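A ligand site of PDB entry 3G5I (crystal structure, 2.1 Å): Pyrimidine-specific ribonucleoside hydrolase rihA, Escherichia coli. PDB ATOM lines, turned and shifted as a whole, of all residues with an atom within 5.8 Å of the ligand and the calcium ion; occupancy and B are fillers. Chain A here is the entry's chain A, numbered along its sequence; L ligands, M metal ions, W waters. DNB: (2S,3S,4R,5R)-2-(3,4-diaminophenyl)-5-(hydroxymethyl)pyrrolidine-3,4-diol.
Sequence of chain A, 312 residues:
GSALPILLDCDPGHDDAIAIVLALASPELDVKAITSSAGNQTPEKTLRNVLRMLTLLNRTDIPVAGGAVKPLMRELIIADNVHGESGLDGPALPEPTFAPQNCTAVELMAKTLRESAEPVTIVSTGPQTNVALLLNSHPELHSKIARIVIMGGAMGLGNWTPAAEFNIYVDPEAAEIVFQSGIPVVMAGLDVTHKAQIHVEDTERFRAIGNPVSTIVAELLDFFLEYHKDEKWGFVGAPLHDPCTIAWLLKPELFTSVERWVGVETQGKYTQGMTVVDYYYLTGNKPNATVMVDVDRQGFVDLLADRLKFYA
Asn 40 touches the calcium ion. The nearest printed residue that does not touch the calcium ion is Gly 126 (4.2 Å).
O of Thr 125 sits close to ND2 of Asn 167. The backbone NH (N) of Asn 40 sits at hydrogen-bond distance from the side-chain carboxylate (OD2) of Asp 11, at 2.7 Å. The backbone NH (N) of Asp 242 is in hydrogen-bond range of the side-chain carboxylate (OD2) of Asp 15 (2.9 Å). ND2 of Asn 40 sits close to OD1 of Asp 16. The side-chain carboxylate of Glu 165 sits at hydrogen-bond distance from the backbone NH of Asn 167, 3.0 Å away. OD1 of Asn 40 is in hydrogen-bond range of NE2 of His 83 (2.9 Å). The backbone carbonyl oxygen (O) of Asn 40 lies within hydrogen-bond range of the backbone NH (N) of Ala 79 (3.3 Å). The side-chain amide oxygen (OD1) of Asn 159 sits at hydrogen-bond distance from the backbone NH (N) of Phe 166 (3.1 Å).
The calcium ion is bound by the backbone carbonyl oxygen (O) of Thr 125, water W1, the side-chain carboxylate (OD1) of Asp 11, the side-chain carboxylate (OD2) of Asp 242, the side-chain carboxylate (OD1) of Asp 16, an oxygen (O2') of the ligand, the side-chain carboxylate (OD2) of Asp 16 and an oxygen (O3') of the ligand.
Water W1 lies within hydrogen-bond range of OD1 of Asn 167 (2.7 Å), OD2 of Asp 11 (2.7 Å), ND2 of Asn 40 (3.1 Å) and N4' of the ligand (3.2 Å).
OE2 of Glu 165 lies within salt-bridge range of N4' of the ligand. The side-chain amide nitrogen of Asn 40 sits close to an oxygen (O2') of the ligand (2.8 Å). O2' of the ligand lies close to OD1 of Asp 15 (2.8 Å). The side-chain amide nitrogen (ND2) of Asn 159 sits at hydrogen-bond distance from an oxygen (O5') of the ligand (2.8 Å). N4' of the ligand lies within hydrogen-bond range of OD1 of Asn 167, at 3.1 Å. SD of Met 151 lies close to O3' of the ligand (3.4 Å).
Ala 79 touches the ligand (CB to C6, 3.8 Å). CG1 of Val 82 touches C4 of the ligand, at 3.7 Å. His 83 touches the ligand (NE2 to C1, 3.4 Å). Phe 166 touches the ligand (CD2 to N4', 3.8 Å). CG of His 241 touches C5' of the ligand, 3.8 Å away. 14 residues have an atom within 4 Å of the ligand: Asp 15, Asp 16, Asn 40, Ala 79, Val 82, His 83, Thr 125, Met 151, Asn 159, Glu 165, Phe 166, Asn 167, His 241 and Asp 242.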
ATOM      1  N   CYS A  10      30.805  -5.941  -1.807  1.00  0.00           N
ATOM      2  CA  CYS A  10      31.100  -5.840  -3.249  1.00  0.00           C
ATOM      3  C   CYS A  10      32.153  -6.851  -3.723  1.00  0.00           C
ATOM      4  O   CYS A  10      32.813  -7.478  -2.919  1.00  0.00           O
ATOM      5  CB  CYS A  10      31.499  -4.394  -3.593  1.00  0.00           C
ATOM      6  SG  CYS A  10      33.036  -3.863  -2.896  1.00  0.00           S
ATOM      7  N   ASP A  11      32.252  -7.036  -5.020  1.00  0.00           N
ATOM      8  CA  ASP A  11      33.124  -8.029  -5.542  1.00  0.00           C
ATOM      9  C   ASP A  11      33.995  -7.519  -6.685  1.00  0.00           C
ATOM     10  O   ASP A  11      33.922  -8.042  -7.786  1.00  0.00           O
ATOM     11  CB  ASP A  11      32.299  -9.272  -5.951  1.00  0.00           C
ATOM     12  CG  ASP A  11      31.348  -8.981  -7.127  1.00  0.00           C
ATOM     13  OD1 ASP A  11      30.848  -7.826  -7.197  1.00  0.00           O
ATOM     14  OD2 ASP A  11      31.093  -9.891  -7.979  1.00  0.00           O
ATOM     15  N   PRO A  12      34.889  -6.535  -6.418  1.00  0.00           N
ATOM     16  CA  PRO A  12      35.591  -5.831  -7.469  1.00  0.00           C
ATOM     17  C   PRO A  12      36.496  -6.728  -8.301  1.00  0.00           C
ATOM     18  O   PRO A  12      37.220  -7.521  -7.720  1.00  0.00           O
ATOM     19  CB  PRO A  12      36.420  -4.771  -6.701  1.00  0.00           C
ATOM     20  CG  PRO A  12      35.900  -4.713  -5.343  1.00  0.00           C
ATOM     21  CD  PRO A  12      35.334  -6.080  -5.081  1.00  0.00           C
ATOM     22  N   GLY A  13      36.426  -6.660  -9.641  1.00  0.00           N
ATOM     23  CA  GLY A  13      35.359  -5.994 -10.436  1.00  0.00           C
ATOM     24  C   GLY A  13      35.438  -4.479 -10.705  1.00  0.00           C
ATOM     25  O   GLY A  13      35.361  -3.641  -9.797  1.00  0.00           O
ATOM     26  N   ASP A  15      33.463  -2.176 -12.051  1.00  0.00           N
ATOM     27  CA  ASP A  15      32.413  -1.261 -11.679  1.00  0.00           C
ATOM     28  C   ASP A  15      32.218  -1.098 -10.164  1.00  0.00           C
ATOM     29  O   ASP A  15      31.983   0.004  -9.695  1.00  0.00           O
ATOM     30  CB  ASP A  15      31.112  -1.529 -12.481  1.00  0.00           C
ATOM     31  CG  ASP A  15      30.556  -2.889 -12.246  1.00  0.00           C
ATOM     32  OD1 ASP A  15      31.333  -3.862 -12.125  1.00  0.00           O
ATOM     33  OD2 ASP A  15      29.319  -2.983 -12.186  1.00  0.00           O
ATOM     34  N   ASP A  16      32.371  -2.167  -9.399  1.00  0.00           N
ATOM     35  CA  ASP A  16      32.466  -2.067  -7.952  1.00  0.00           C
ATOM     36  C   ASP A  16      33.539  -1.073  -7.552  1.00  0.00           C
ATOM     37  O   ASP A  16      33.294  -0.225  -6.685  1.00  0.00           O
ATOM     38  CB  ASP A  16      32.868  -3.422  -7.317  1.00  0.00           C
ATOM     39  CG  ASP A  16      31.932  -4.560  -7.728  1.00  0.00           C
ATOM     40  OD1 ASP A  16      32.161  -5.197  -8.806  1.00  0.00           O
ATOM     41  OD2 ASP A  16      30.979  -4.804  -6.959  1.00  0.00           O
ATOM     42  N   ASN A  40      32.280 -11.958  -9.219  1.00  0.00           N
ATOM     43  CA  ASN A  40      33.191 -11.462 -10.287  1.00  0.00           C
ATOM     44  C   ASN A  40      34.517 -12.243 -10.296  1.00  0.00           C
ATOM     45  O   ASN A  40      35.039 -12.556 -11.378  1.00  0.00           O
ATOM     46  CB  ASN A  40      33.464  -9.933 -10.198  1.00  0.00           C
ATOM     47  CG  ASN A  40      32.389  -9.071 -10.918  1.00  0.00           C
ATOM     48  OD1 ASN A  40      31.687  -9.555 -11.833  1.00  0.00           O
ATOM     49  ND2 ASN A  40      32.214  -7.806 -10.467  1.00  0.00           N
ATOM     50  N   ALA A  79      32.577 -14.250 -12.861  1.00  0.00           N
ATOM     51  CA  ALA A  79      32.578 -13.470 -14.115  1.00  0.00           C
ATOM     52  C   ALA A  79      34.042 -13.289 -14.579  1.00  0.00           C
ATOM     53  O   ALA A  79      34.643 -12.196 -14.480  1.00  0.00           O
ATOM     54  CB  ALA A  79      31.844 -12.149 -13.941  1.00  0.00           C
ATOM     55  N   VAL A  82      35.247 -11.639 -18.630  1.00  0.00           N
ATOM     56  CA  VAL A  82      34.585 -10.322 -18.680  1.00  0.00           C
ATOM     57  C   VAL A  82      35.417  -9.244 -17.938  1.00  0.00           C
ATOM     58  O   VAL A  82      35.682  -8.157 -18.499  1.00  0.00           O
ATOM     59  CB  VAL A  82      33.146 -10.369 -18.048  1.00  0.00           C
ATOM     60  CG1 VAL A  82      32.562  -8.975 -17.910  1.00  0.00           C
ATOM     61  CG2 VAL A  82      32.228 -11.284 -18.846  1.00  0.00           C
ATOM     62  N   HIS A  83      35.816  -9.573 -16.708  1.00  0.00           N
ATOM     63  CA  HIS A  83      36.582  -8.703 -15.790  1.00  0.00           C
ATOM     64  C   HIS A  83      38.105  -8.986 -15.800  1.00  0.00           C
ATOM     65  O   HIS A  83      38.884  -8.363 -15.043  1.00  0.00           O
ATOM     66  CB  HIS A  83      36.020  -8.839 -14.367  1.00  0.00           C
ATOM     67  CG  HIS A  83      34.622  -8.343 -14.231  1.00  0.00           C
ATOM     68  ND1 HIS A  83      34.319  -7.008 -14.016  1.00  0.00           N
ATOM     69  CD2 HIS A  83      33.426  -8.985 -14.331  1.00  0.00           C
ATOM     70  CE1 HIS A  83      33.003  -6.854 -13.968  1.00  0.00           C
ATOM     71  NE2 HIS A  83      32.439  -8.036 -14.158  1.00  0.00           N
ATOM     72  N   THR A 125      26.802  -5.002  -4.080  1.00  0.00           N
ATOM     73  CA  THR A 125      26.975  -4.911  -5.517  1.00  0.00           C
ATOM     74  C   THR A 125      27.606  -6.165  -6.128  1.00  0.00           C
ATOM     75  O   THR A 125      27.965  -6.188  -7.307  1.00  0.00           O
ATOM     76  CB  THR A 125      27.789  -3.602  -5.900  1.00  0.00           C
ATOM     77  OG1 THR A 125      29.126  -3.636  -5.371  1.00  0.00           O
ATOM     78  CG2 THR A 125      27.093  -2.422  -5.376  1.00  0.00           C
ATOM     79  N   GLY A 126      27.733  -7.201  -5.305  1.00  0.00           N
ATOM     80  CA  GLY A 126      27.965  -8.513  -5.816  1.00  0.00           C
ATOM     81  C   GLY A 126      26.801  -9.430  -5.497  1.00  0.00           C
ATOM     82  O   GLY A 126      25.731  -8.972  -5.093  1.00  0.00           O
ATOM     83  N   MET A 151      22.970  -3.859  -6.596  1.00  0.00           N
ATOM     84  CA  MET A 151      23.047  -3.966  -8.035  1.00  0.00           C
ATOM     85  C   MET A 151      22.796  -5.457  -8.335  1.00  0.00           C
ATOM     86  O   MET A 151      23.493  -6.375  -7.828  1.00  0.00           O
ATOM     87  CB  MET A 151      24.388  -3.475  -8.584  1.00  0.00           C
ATOM     88  CG  MET A 151      24.362  -3.380 -10.132  1.00  0.00           C
ATOM     89  SD  MET A 151      24.403  -5.033 -10.866  1.00  0.00           S
ATOM     90  CE  MET A 151      23.280  -4.774 -12.251  1.00  0.00           C
ATOM     91  N   ASN A 159      21.558 -11.008 -18.351  1.00  0.00           N
ATOM     92  CA  ASN A 159      22.841 -10.961 -19.041  1.00  0.00           C
ATOM     93  C   ASN A 159      23.692 -12.200 -18.821  1.00  0.00           C
ATOM     94  O   ASN A 159      24.784 -12.314 -19.391  1.00  0.00           O
ATOM     95  CB  ASN A 159      23.635  -9.646 -18.706  1.00  0.00           C
ATOM     96  CG  ASN A 159      24.069  -9.554 -17.216  1.00  0.00           C
ATOM     97  OD1 ASN A 159      23.693 -10.393 -16.374  1.00  0.00           O
ATOM     98  ND2 ASN A 159      24.905  -8.514 -16.893  1.00  0.00           N
ATOM     99  N   TRP A 160      23.201 -13.140 -18.012  1.00  0.00           N
ATOM    100  CA  TRP A 160      23.987 -14.320 -17.732  1.00  0.00           C
ATOM    101  C   TRP A 160      23.370 -15.617 -18.332  1.00  0.00           C
ATOM    102  O   TRP A 160      24.035 -16.362 -19.103  1.00  0.00           O
ATOM    103  CB  TRP A 160      24.225 -14.456 -16.232  1.00  0.00           C
ATOM    104  CG  TRP A 160      25.342 -15.443 -15.979  1.00  0.00           C
ATOM    105  CD1 TRP A 160      25.225 -16.702 -15.436  1.00  0.00           C
ATOM    106  CD2 TRP A 160      26.737 -15.267 -16.314  1.00  0.00           C
ATOM    107  NE1 TRP A 160      26.474 -17.303 -15.434  1.00  0.00           N
ATOM    108  CE2 TRP A 160      27.408 -16.441 -15.945  1.00  0.00           C
ATOM    109  CE3 TRP A 160      27.473 -14.218 -16.919  1.00  0.00           C
ATOM    110  CZ2 TRP A 160      28.804 -16.636 -16.159  1.00  0.00           C
ATOM    111  CZ3 TRP A 160      28.862 -14.374 -17.108  1.00  0.00           C
ATOM    112  CH2 TRP A 160      29.507 -15.584 -16.740  1.00  0.00           C
ATOM    113  N   GLU A 165      20.162 -12.230 -14.343  1.00  0.00           N
ATOM    114  CA  GLU A 165      21.343 -11.391 -14.263  1.00  0.00           C
ATOM    115  C   GLU A 165      22.369 -12.085 -13.376  1.00  0.00           C
ATOM    116  O   GLU A 165      22.022 -12.833 -12.499  1.00  0.00           O
ATOM    117  CB  GLU A 165      20.955  -9.964 -13.794  1.00  0.00           C
ATOM    118  CG  GLU A 165      22.120  -8.951 -13.577  1.00  0.00           C
ATOM    119  CD  GLU A 165      22.851  -9.153 -12.251  1.00  0.00           C
ATOM    120  OE1 GLU A 165      22.217  -9.557 -11.262  1.00  0.00           O
ATOM    121  OE2 GLU A 165      24.061  -8.886 -12.194  1.00  0.00           O
ATOM    122  N   PHE A 166      23.657 -11.853 -13.616  1.00  0.00           N
ATOM    123  CA  PHE A 166      24.740 -12.597 -12.971  1.00  0.00           C
ATOM    124  C   PHE A 166      24.741 -12.641 -11.434  1.00  0.00           C
ATOM    125  O   PHE A 166      24.823 -13.677 -10.829  1.00  0.00           O
ATOM    126  CB  PHE A 166      26.077 -12.021 -13.454  1.00  0.00           C
ATOM    127  CG  PHE A 166      27.273 -12.649 -12.771  1.00  0.00           C
ATOM    128  CD1 PHE A 166      27.844 -13.822 -13.283  1.00  0.00           C
ATOM    129  CD2 PHE A 166      27.857 -12.045 -11.634  1.00  0.00           C
ATOM    130  CE1 PHE A 166      28.948 -14.431 -12.665  1.00  0.00           C
ATOM    131  CE2 PHE A 166      28.983 -12.637 -10.987  1.00  0.00           C
ATOM    132  CZ  PHE A 166      29.538 -13.832 -11.516  1.00  0.00           C
ATOM    133  N   ASN A 167      24.740 -11.482 -10.791  1.00  0.00           N
ATOM    134  CA  ASN A 167      24.796 -11.392  -9.322  1.00  0.00           C
ATOM    135  C   ASN A 167      23.723 -12.211  -8.681  1.00  0.00           C
ATOM    136  O   ASN A 167      23.952 -12.883  -7.676  1.00  0.00           O
ATOM    137  CB  ASN A 167      24.616  -9.972  -8.846  1.00  0.00           C
ATOM    138  CG  ASN A 167      25.838  -9.152  -9.013  1.00  0.00           C
ATOM    139  OD1 ASN A 167      26.937  -9.624  -9.461  1.00  0.00           O
ATOM    140  ND2 ASN A 167      25.691  -7.876  -8.662  1.00  0.00           N
ATOM    141  N   LEU A 190      19.345  -4.491 -14.514  1.00  0.00           N
ATOM    142  CA  LEU A 190      19.798  -4.215 -15.875  1.00  0.00           C
ATOM    143  C   LEU A 190      18.877  -3.190 -16.576  1.00  0.00           C
ATOM    144  O   LEU A 190      19.288  -2.475 -17.470  1.00  0.00           O
ATOM    145  CB  LEU A 190      19.871  -5.507 -16.666  1.00  0.00           C
ATOM    146  CG  LEU A 190      20.923  -6.484 -16.140  1.00  0.00           C
ATOM    147  CD1 LEU A 190      20.934  -7.744 -17.014  1.00  0.00           C
ATOM    148  CD2 LEU A 190      22.347  -5.861 -16.014  1.00  0.00           C
ATOM    149  N   PHE A 224      36.833  -2.375 -20.235  1.00  0.00           N
ATOM    150  CA  PHE A 224      35.458  -2.749 -20.590  1.00  0.00           C
ATOM    151  C   PHE A 224      35.042  -2.436 -22.024  1.00  0.00           C
ATOM    152  O   PHE A 224      33.831  -2.456 -22.310  1.00  0.00           O
ATOM    153  CB  PHE A 224      34.436  -2.023 -19.733  1.00  0.00           C
ATOM    154  CG  PHE A 224      34.244  -2.573 -18.363  1.00  0.00           C
ATOM    155  CD1 PHE A 224      34.010  -3.930 -18.162  1.00  0.00           C
ATOM    156  CD2 PHE A 224      34.234  -1.701 -17.261  1.00  0.00           C
ATOM    157  CE1 PHE A 224      33.804  -4.422 -16.872  1.00  0.00           C
ATOM    158  CE2 PHE A 224      34.025  -2.160 -15.974  1.00  0.00           C
ATOM    159  CZ  PHE A 224      33.805  -3.533 -15.760  1.00  0.00           C
ATOM    160  N   HIS A 241      27.412  -0.518 -14.064  1.00  0.00           N
ATOM    161  CA  HIS A 241      26.349  -1.075 -13.234  1.00  0.00           C
ATOM    162  C   HIS A 241      26.422  -0.599 -11.780  1.00  0.00           C
ATOM    163  O   HIS A 241      25.522   0.087 -11.266  1.00  0.00           O
ATOM    164  CB  HIS A 241      26.359  -2.635 -13.279  1.00  0.00           C
ATOM    165  CG  HIS A 241      26.359  -3.206 -14.678  1.00  0.00           C
ATOM    166  ND1 HIS A 241      25.196  -3.408 -15.390  1.00  0.00           N
ATOM    167  CD2 HIS A 241      27.370  -3.643 -15.458  1.00  0.00           C
ATOM    168  CE1 HIS A 241      25.496  -3.952 -16.566  1.00  0.00           C
ATOM    169  NE2 HIS A 241      26.811  -4.054 -16.644  1.00  0.00           N
ATOM    170  N   ASP A 242      27.508  -0.975 -11.102  1.00  0.00           N
ATOM    171  CA  ASP A 242      27.537  -0.817  -9.636  1.00  0.00           C
ATOM    172  C   ASP A 242      27.425   0.643  -9.112  1.00  0.00           C
ATOM    173  O   ASP A 242      26.691   0.916  -8.118  1.00  0.00           O
ATOM    174  CB  ASP A 242      28.766  -1.571  -9.088  1.00  0.00           C
ATOM    175  CG  ASP A 242      28.640  -3.083  -9.307  1.00  0.00           C
ATOM    176  OD1 ASP A 242      27.505  -3.520  -9.690  1.00  0.00           O
ATOM    177  OD2 ASP A 242      29.612  -3.853  -9.080  1.00  0.00           O
HETATM  178  O2' DNB L   1      30.105  -6.207 -11.275  1.00  0.00           O
HETATM  179  C2' DNB L   1      29.131  -6.401 -12.327  1.00  0.00           C
HETATM  180  C3' DNB L   1      27.744  -5.986 -11.798  1.00  0.00           C
HETATM  181  O3' DNB L   1      27.672  -5.857 -10.362  1.00  0.00           O
HETATM  182  C1' DNB L   1      29.014  -7.892 -12.707  1.00  0.00           C
HETATM  183  N4' DNB L   1      27.682  -8.256 -12.198  1.00  0.00           N
HETATM  184  C4' DNB L   1      26.794  -7.110 -12.262  1.00  0.00           C
HETATM  185  C5' DNB L   1      26.228  -6.834 -13.681  1.00  0.00           C
HETATM  186  O5' DNB L   1      25.599  -8.016 -14.185  1.00  0.00           O
HETATM  187  C1  DNB L   1      29.048  -8.275 -14.160  1.00  0.00           C
HETATM  188  C6  DNB L   1      28.978  -9.643 -14.451  1.00  0.00           C
HETATM  189  C5  DNB L   1      28.985 -10.164 -15.745  1.00  0.00           C
HETATM  190  C4  DNB L   1      29.040  -9.264 -16.817  1.00  0.00           C
HETATM  191  C3  DNB L   1      29.103  -7.883 -16.584  1.00  0.00           C
HETATM  192  N3  DNB L   1      29.162  -7.085 -17.669  1.00  0.00           N
HETATM  193  C2  DNB L   1      29.085  -7.387 -15.253  1.00  0.00           C
HETATM  194 CA    CA M   1      29.871  -6.255  -8.742  1.00  0.00          CA
HETATM  195  O   HOH W   1      29.352  -8.450  -9.525  1.00  0.00           O
